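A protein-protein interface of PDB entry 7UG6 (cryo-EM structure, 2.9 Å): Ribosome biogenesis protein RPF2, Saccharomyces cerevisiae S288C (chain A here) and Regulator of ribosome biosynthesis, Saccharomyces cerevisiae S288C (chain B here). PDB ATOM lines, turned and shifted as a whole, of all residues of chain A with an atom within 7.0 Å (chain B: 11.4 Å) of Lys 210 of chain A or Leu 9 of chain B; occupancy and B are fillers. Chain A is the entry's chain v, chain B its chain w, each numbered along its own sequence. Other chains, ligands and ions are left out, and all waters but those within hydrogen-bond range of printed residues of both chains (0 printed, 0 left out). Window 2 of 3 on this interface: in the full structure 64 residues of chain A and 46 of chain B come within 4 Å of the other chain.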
ATOM      1  N   SER A 208      12.241 -25.864  -2.334  1.00  0.00           N
ATOM      2  CA  SER A 208      12.641 -24.679  -1.601  1.00  0.00           C
ATOM      3  C   SER A 208      14.107 -24.765  -1.220  1.00  0.00           C
ATOM      4  O   SER A 208      14.539 -25.695  -0.534  1.00  0.00           O
ATOM      5  CB  SER A 208      11.802 -24.488  -0.353  1.00  0.00           C
ATOM      6  OG  SER A 208      10.432 -24.531  -0.680  1.00  0.00           O
ATOM      7  N   TYR A 209      14.860 -23.762  -1.649  1.00  0.00           N
ATOM      8  CA  TYR A 209      16.251 -23.627  -1.279  1.00  0.00           C
ATOM      9  C   TYR A 209      16.391 -22.409  -0.384  1.00  0.00           C
ATOM     10  O   TYR A 209      15.662 -21.426  -0.525  1.00  0.00           O
ATOM     11  CB  TYR A 209      17.152 -23.494  -2.506  1.00  0.00           C
ATOM     12  CG  TYR A 209      17.172 -24.729  -3.359  1.00  0.00           C
ATOM     13  CD1 TYR A 209      16.737 -24.699  -4.667  1.00  0.00           C
ATOM     14  CD2 TYR A 209      17.595 -25.932  -2.843  1.00  0.00           C
ATOM     15  CE1 TYR A 209      16.751 -25.828  -5.446  1.00  0.00           C
ATOM     16  CE2 TYR A 209      17.604 -27.075  -3.609  1.00  0.00           C
ATOM     17  CZ  TYR A 209      17.179 -27.020  -4.913  1.00  0.00           C
ATOM     18  OH  TYR A 209      17.187 -28.159  -5.688  1.00  0.00           O
ATOM     19  N   LYS A 210      17.320 -22.508   0.562  1.00  0.00           N
ATOM     20  CA  LYS A 210      17.562 -21.427   1.498  1.00  0.00           C
ATOM     21  C   LYS A 210      17.982 -20.186   0.729  1.00  0.00           C
ATOM     22  O   LYS A 210      18.728 -20.269  -0.247  1.00  0.00           O
ATOM     23  CB  LYS A 210      18.687 -21.790   2.459  1.00  0.00           C
ATOM     24  CG  LYS A 210      18.505 -23.035   3.330  1.00  0.00           C
ATOM     25  CD  LYS A 210      17.483 -22.969   4.436  1.00  0.00           C
ATOM     26  CE  LYS A 210      16.132 -23.506   4.014  1.00  0.00           C
ATOM     27  NZ  LYS A 210      15.199 -23.533   5.151  1.00  0.00           N
ATOM     28  N   SER A 211      17.523 -19.026   1.181  1.00  0.00           N
ATOM     29  CA  SER A 211      18.014 -17.778   0.610  1.00  0.00           C
ATOM     30  C   SER A 211      18.031 -16.747   1.722  1.00  0.00           C
ATOM     31  O   SER A 211      16.989 -16.449   2.314  1.00  0.00           O
ATOM     32  CB  SER A 211      17.153 -17.321  -0.554  1.00  0.00           C
ATOM     33  OG  SER A 211      15.853 -16.979  -0.120  1.00  0.00           O
ATOM     34  N   ASP A 212      19.206 -16.199   1.993  1.00  0.00           N
ATOM     35  CA  ASP A 212      19.403 -15.325   3.137  1.00  0.00           C
ATOM     36  C   ASP A 212      19.131 -13.863   2.821  1.00  0.00           C
ATOM     37  O   ASP A 212      19.776 -12.975   3.390  1.00  0.00           O
ATOM     38  CB  ASP A 212      20.803 -15.549   3.708  1.00  0.00           C
ATOM     39  CG  ASP A 212      21.894 -15.216   2.731  1.00  0.00           C
ATOM     40  OD1 ASP A 212      21.580 -14.847   1.577  1.00  0.00           O
ATOM     41  OD2 ASP A 212      23.073 -15.342   3.120  1.00  0.00           O
ATOM     42  N   GLN A 213      18.193 -13.594   1.913  1.00  0.00           N
ATOM     43  CA  GLN A 213      17.745 -12.222   1.704  1.00  0.00           C
ATOM     44  C   GLN A 213      16.853 -11.756   2.844  1.00  0.00           C
ATOM     45  O   GLN A 213      17.207 -10.836   3.590  1.00  0.00           O
ATOM     46  CB  GLN A 213      17.016 -12.114   0.371  1.00  0.00           C
ATOM     47  CG  GLN A 213      17.810 -12.677  -0.774  1.00  0.00           C
ATOM     48  CD  GLN A 213      19.243 -12.197  -0.749  1.00  0.00           C
ATOM     49  OE1 GLN A 213      20.156 -12.953  -0.424  1.00  0.00           O
ATOM     50  NE2 GLN A 213      19.448 -10.929  -1.092  1.00  0.00           N
ATOM     51  N   GLY A 215      16.004 -13.691   5.367  1.00  0.00           N
ATOM     52  CA  GLY A 215      16.378 -14.410   6.557  1.00  0.00           C
ATOM     53  C   GLY A 215      16.028 -15.880   6.473  1.00  0.00           C
ATOM     54  O   GLY A 215      15.823 -16.449   5.399  1.00  0.00           O
ATOM     55  N   LYS A 216      15.961 -16.501   7.646  1.00  0.00           N
ATOM     56  CA  LYS A 216      15.604 -17.902   7.773  1.00  0.00           C
ATOM     57  C   LYS A 216      14.130 -18.129   7.476  1.00  0.00           C
ATOM     58  O   LYS A 216      13.730 -19.258   7.179  1.00  0.00           O
ATOM     59  CB  LYS A 216      15.915 -18.374   9.199  1.00  0.00           C
ATOM     60  CG  LYS A 216      15.861 -19.878   9.466  1.00  0.00           C
ATOM     61  CD  LYS A 216      16.251 -20.742   8.264  1.00  0.00           C
ATOM     62  CE  LYS A 216      17.769 -20.651   8.027  1.00  0.00           C
ATOM     63  NZ  LYS A 216      18.371 -21.736   7.210  1.00  0.00           N
ATOM     64  N   LEU A 218      11.830 -16.939   5.104  1.00  0.00           N
ATOM     65  CA  LEU A 218      11.249 -17.112   3.776  1.00  0.00           C
ATOM     66  C   LEU A 218      12.270 -17.648   2.787  1.00  0.00           C
ATOM     67  O   LEU A 218      13.283 -16.982   2.514  1.00  0.00           O
ATOM     68  CB  LEU A 218      10.619 -15.791   3.333  1.00  0.00           C
ATOM     69  CG  LEU A 218      11.351 -14.458   3.147  1.00  0.00           C
ATOM     70  CD1 LEU A 218      12.041 -14.275   1.818  1.00  0.00           C
ATOM     71  CD2 LEU A 218      10.364 -13.337   3.383  1.00  0.00           C
ATOM     72  N   PRO A 219      12.087 -18.859   2.282  1.00  0.00           N
ATOM     73  CA  PRO A 219      13.091 -19.469   1.416  1.00  0.00           C
ATOM     74  C   PRO A 219      12.900 -19.043  -0.031  1.00  0.00           C
ATOM     75  O   PRO A 219      11.933 -18.372  -0.387  1.00  0.00           O
ATOM     76  CB  PRO A 219      12.812 -20.964   1.584  1.00  0.00           C
ATOM     77  CG  PRO A 219      11.375 -21.032   1.816  1.00  0.00           C
ATOM     78  CD  PRO A 219      10.994 -19.797   2.578  1.00  0.00           C
ATOM     79  N   ARG A 220      13.853 -19.440  -0.861  1.00  0.00           N
ATOM     80  CA  ARG A 220      13.721 -19.222  -2.285  1.00  0.00           C
ATOM     81  C   ARG A 220      13.198 -20.495  -2.903  1.00  0.00           C
ATOM     82  O   ARG A 220      13.710 -21.585  -2.648  1.00  0.00           O
ATOM     83  CB  ARG A 220      15.042 -18.856  -2.936  1.00  0.00           C
ATOM     84  CG  ARG A 220      14.859 -18.185  -4.260  1.00  0.00           C
ATOM     85  CD  ARG A 220      15.044 -19.083  -5.440  1.00  0.00           C
ATOM     86  NE  ARG A 220      15.031 -18.282  -6.657  1.00  0.00           N
ATOM     87  CZ  ARG A 220      15.064 -18.782  -7.883  1.00  0.00           C
ATOM     88  NH1 ARG A 220      15.092 -20.097  -8.065  1.00  0.00           N
ATOM     89  NH2 ARG A 220      15.050 -17.966  -8.924  1.00  0.00           N
ATOM     90  N   LEU B   9      19.162 -17.237  -6.070  1.00  0.00           N
ATOM     91  CA  LEU B   9      19.114 -16.691  -4.713  1.00  0.00           C
ATOM     92  C   LEU B   9      18.248 -15.436  -4.458  1.00  0.00           C
ATOM     93  O   LEU B   9      17.899 -15.181  -3.314  1.00  0.00           O
ATOM     94  CB  LEU B   9      20.537 -16.406  -4.222  1.00  0.00           C
ATOM     95  CG  LEU B   9      21.367 -17.619  -3.778  1.00  0.00           C
ATOM     96  CD1 LEU B   9      22.585 -17.178  -2.998  1.00  0.00           C
ATOM     97  CD2 LEU B   9      20.547 -18.594  -2.956  1.00  0.00           C
ATOM     98  N   PRO B  10      17.930 -14.628  -5.470  1.00  0.00           N
ATOM     99  CA  PRO B  10      16.934 -13.575  -5.247  1.00  0.00           C
ATOM    100  C   PRO B  10      15.574 -14.146  -4.895  1.00  0.00           C
ATOM    101  O   PRO B  10      15.140 -15.154  -5.452  1.00  0.00           O
ATOM    102  CB  PRO B  10      16.899 -12.840  -6.584  1.00  0.00           C
ATOM    103  CG  PRO B  10      18.268 -12.963  -7.073  1.00  0.00           C
ATOM    104  CD  PRO B  10      18.707 -14.345  -6.691  1.00  0.00           C
ATOM    105  N   VAL B  11      14.891 -13.474  -3.969  1.00  0.00           N
ATOM    106  CA  VAL B  11      13.552 -13.862  -3.560  1.00  0.00           C
ATOM    107  C   VAL B  11      12.571 -12.696  -3.630  1.00  0.00           C
ATOM    108  O   VAL B  11      11.362 -12.921  -3.745  1.00  0.00           O
ATOM    109  CB  VAL B  11      13.584 -14.467  -2.142  1.00  0.00           C
ATOM    110  CG1 VAL B  11      13.970 -13.422  -1.138  1.00  0.00           C
ATOM    111  CG2 VAL B  11      12.271 -15.072  -1.783  1.00  0.00           C
ATOM    112  N   THR B  12      13.057 -11.463  -3.598  1.00  0.00           N
ATOM    113  CA  THR B  12      12.201 -10.292  -3.672  1.00  0.00           C
ATOM    114  C   THR B  12      11.963  -9.900  -5.122  1.00  0.00           C
ATOM    115  O   THR B  12      12.498  -8.889  -5.586  1.00  0.00           O
ATOM    116  CB  THR B  12      12.846  -9.145  -2.906  1.00  0.00           C
ATOM    117  OG1 THR B  12      14.234  -9.084  -3.251  1.00  0.00           O
ATOM    118  CG2 THR B  12      12.732  -9.386  -1.414  1.00  0.00           C
ATOM    119  N   VAL B  13      11.183 -10.688  -5.852  1.00  0.00           N
ATOM    120  CA  VAL B  13      10.963 -10.423  -7.270  1.00  0.00           C
ATOM    121  C   VAL B  13       9.653  -9.662  -7.448  1.00  0.00           C
ATOM    122  O   VAL B  13       8.643  -9.983  -6.817  1.00  0.00           O
ATOM    123  CB  VAL B  13      10.992 -11.720  -8.092  1.00  0.00           C
ATOM    124  CG1 VAL B  13       9.857 -12.649  -7.728  1.00  0.00           C
ATOM    125  CG2 VAL B  13      10.969 -11.406  -9.586  1.00  0.00           C
ATOM    126  N   ARG B  55       7.061 -19.697 -11.531  1.00  0.00           N
ATOM    127  CA  ARG B  55       7.927 -19.682 -10.362  1.00  0.00           C
ATOM    128  C   ARG B  55       7.832 -18.345  -9.665  1.00  0.00           C
ATOM    129  O   ARG B  55       7.802 -18.283  -8.437  1.00  0.00           O
ATOM    130  CB  ARG B  55       9.380 -19.983 -10.747  1.00  0.00           C
ATOM    131  CG  ARG B  55      10.385 -19.817  -9.602  1.00  0.00           C
ATOM    132  CD  ARG B  55      10.982 -18.426  -9.618  1.00  0.00           C
ATOM    133  NE  ARG B  55      11.778 -18.112  -8.447  1.00  0.00           N
ATOM    134  CZ  ARG B  55      11.949 -16.876  -7.995  1.00  0.00           C
ATOM    135  NH1 ARG B  55      11.355 -15.863  -8.605  1.00  0.00           N
ATOM    136  NH2 ARG B  55      12.687 -16.647  -6.922  1.00  0.00           N
ATOM    137  N   ASP B  56       7.822 -17.259 -10.431  1.00  0.00           N
ATOM    138  CA  ASP B  56       7.715 -15.945  -9.813  1.00  0.00           C
ATOM    139  C   ASP B  56       6.399 -15.806  -9.070  1.00  0.00           C
ATOM    140  O   ASP B  56       6.364 -15.327  -7.929  1.00  0.00           O
ATOM    141  CB  ASP B  56       7.858 -14.857 -10.868  1.00  0.00           C
ATOM    142  CG  ASP B  56       9.287 -14.380 -11.010  1.00  0.00           C
ATOM    143  OD1 ASP B  56       9.540 -13.471 -11.830  1.00  0.00           O
ATOM    144  OD2 ASP B  56      10.157 -14.920 -10.298  1.00  0.00           O
ATOM    145  N   GLN B  59       6.568 -17.765  -5.972  1.00  0.00           N
ATOM    146  CA  GLN B  59       7.462 -17.139  -5.011  1.00  0.00           C
ATOM    147  C   GLN B  59       6.742 -16.059  -4.233  1.00  0.00           C
ATOM    148  O   GLN B  59       6.833 -16.002  -3.005  1.00  0.00           O
ATOM    149  CB  GLN B  59       8.670 -16.555  -5.725  1.00  0.00           C
ATOM    150  CG  GLN B  59       9.675 -15.938  -4.800  1.00  0.00           C
ATOM    151  CD  GLN B  59      10.001 -16.823  -3.637  1.00  0.00           C
ATOM    152  OE1 GLN B  59      10.760 -17.772  -3.769  1.00  0.00           O
ATOM    153  NE2 GLN B  59       9.439 -16.514  -2.483  1.00  0.00           N
ATOM    154  N   ILE B  62       4.116 -17.827  -1.851  1.00  0.00           N
ATOM    155  CA  ILE B  62       4.717 -18.401  -0.654  1.00  0.00           C
ATOM    156  C   ILE B  62       5.234 -17.300   0.259  1.00  0.00           C
ATOM    157  O   ILE B  62       5.163 -17.413   1.484  1.00  0.00           O
ATOM    158  CB  ILE B  62       5.821 -19.399  -1.046  1.00  0.00           C
ATOM    159  CG1 ILE B  62       5.206 -20.727  -1.480  1.00  0.00           C
ATOM    160  CG2 ILE B  62       6.786 -19.638   0.088  1.00  0.00           C
ATOM    161  CD1 ILE B  62       4.685 -21.543  -0.351  1.00  0.00           C
ATOM    162  N   ASN B  63       5.743 -16.211  -0.317  1.00  0.00           N
ATOM    163  CA  ASN B  63       6.156 -15.086   0.509  1.00  0.00           C
ATOM    164  C   ASN B  63       4.998 -14.553   1.326  1.00  0.00           C
ATOM    165  O   ASN B  63       5.149 -14.294   2.524  1.00  0.00           O
ATOM    166  CB  ASN B  63       6.723 -13.974  -0.361  1.00  0.00           C
ATOM    167  CG  ASN B  63       8.112 -14.265  -0.825  1.00  0.00           C
ATOM    168  OD1 ASN B  63       8.633 -15.348  -0.591  1.00  0.00           O
ATOM    169  ND2 ASN B  63       8.727 -13.305  -1.499  1.00  0.00           N
ATOM    170  N   LEU B  66       3.786 -17.756   3.939  1.00  0.00           N
ATOM    171  CA  LEU B  66       4.599 -17.974   5.124  1.00  0.00           C
ATOM    172  C   LEU B  66       4.548 -16.784   6.051  1.00  0.00           C
ATOM    173  O   LEU B  66       4.761 -16.935   7.253  1.00  0.00           O
ATOM    174  CB  LEU B  66       6.044 -18.264   4.734  1.00  0.00           C
ATOM    175  CG  LEU B  66       6.313 -19.631   4.120  1.00  0.00           C
ATOM    176  CD1 LEU B  66       7.767 -19.950   4.208  1.00  0.00           C
ATOM    177  CD2 LEU B  66       5.507 -20.691   4.820  1.00  0.00           C
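The guanidinium group (NE) of Arg 220 of chain A sits close to the backbone carbonyl oxygen (O) of Pro 10 of chain B (3.4 Å).
The guanidinium group of Arg 220 of chain A lies close to the guanidinium group of Arg 55 of chain B (2.9 Å).
The backbone NH of Tyr 209 of chain A sits at hydrogen-bond distance from the backbone carbonyl oxygen of Arg 220 of chain A.
OG of Ser 211 of chain A lies within hydrogen-bond range of N of Arg 220 of chain A, 3.3 Å away.
OD1 of Asp 212 of chain A lies close to OE1 of Gln 213 of chain A (3.1 Å).
NH2 of Arg 55 of chain B is in hydrogen-bond range of O of Pro 10 of chain B, at 3.2 Å.
The backbone carbonyl oxygen (O) of Val 11 of chain B sits at hydrogen-bond distance from the side-chain amide nitrogen (ND2) of Asn 63 of chain B (3.5 Å).
O of Gln 59 of chain B sits close to OD1 of Asn 63 of chain B.
No residue of chain B comes within 4 Å of Ser 208 of chain A.
Lys 210 of chain A touches just one residue of chain B: Leu 9 (3.7 Å).
No residue of chain B comes within 4 Å of Asp 212 of chain A.
Of the printed residues of chain B, Gln 213 of chain A touches Leu 9 (3.6 Å) and Val 11 (3.6 Å).
Pro 219 of chain A touches just these residues of chain B: Val 11 (3.6 Å), Gln 59 (3.6 Å) and Leu 66 (3.6 Å).
Of chain B, only Pro 10, Arg 55 and Gln 59 come within 4 Å of Arg 220 of chain A.
Of chain A, only Lys 210, Ser 211 and Gln 213 come within 4 Å of Leu 9 of chain B.
Of the printed residues of chain A, Pro 10 of chain B touches Arg 220 (3.3 Å).
Of the printed residues of chain A, Arg 55 of chain B touches Arg 220.
Asp 56 of chain B touches none of the printed residues of chain A.
The nearest printed residue of chain A that does not touch Arg 55 of chain B is Pro 219 of chain A (6.8 Å).
Hydrophobic or aromatic side chains of chain A within 4 Å of the printed part of chain B: Leu 218 and Pro 219.
Hydrophobic or aromatic side chains of chain B within 4 Å of the printed part of chain A: Leu 9, Val 11 and Leu 66.
Among the printed residues, 12 pairs touch across the chains.
Among the printed residues, no Asp or Glu carboxylate lies within 4 Å of a Lys or Arg side-chain nitrogen of the other chain.
Among the printed residues, pairs that only touch across the chains: Lys 210 of chain A with Leu 9 of chain B (3.7 Å), Ser 211 of chain A with Leu 9 of chain B (3.6 Å), Ser 211 of chain A with Val 11 of chain B (3.9 Å), Gln 213 of chain A with Leu 9 of chain B (3.6 Å), Gln 213 of chain A with Val 11 of chain B (3.6 Å), Leu 218 of chain A with Val 11 of chain B (3.6 Å), Pro 219 of chain A with Val 11 of chain B (3.6 Å), Pro 219 of chain A with Gln 59 of chain B (3.6 Å), Pro 219 of chain A with Leu 66 of chain B (3.6 Å) and Arg 220 of chain A with Gln 59 of chain B (3.6 Å).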
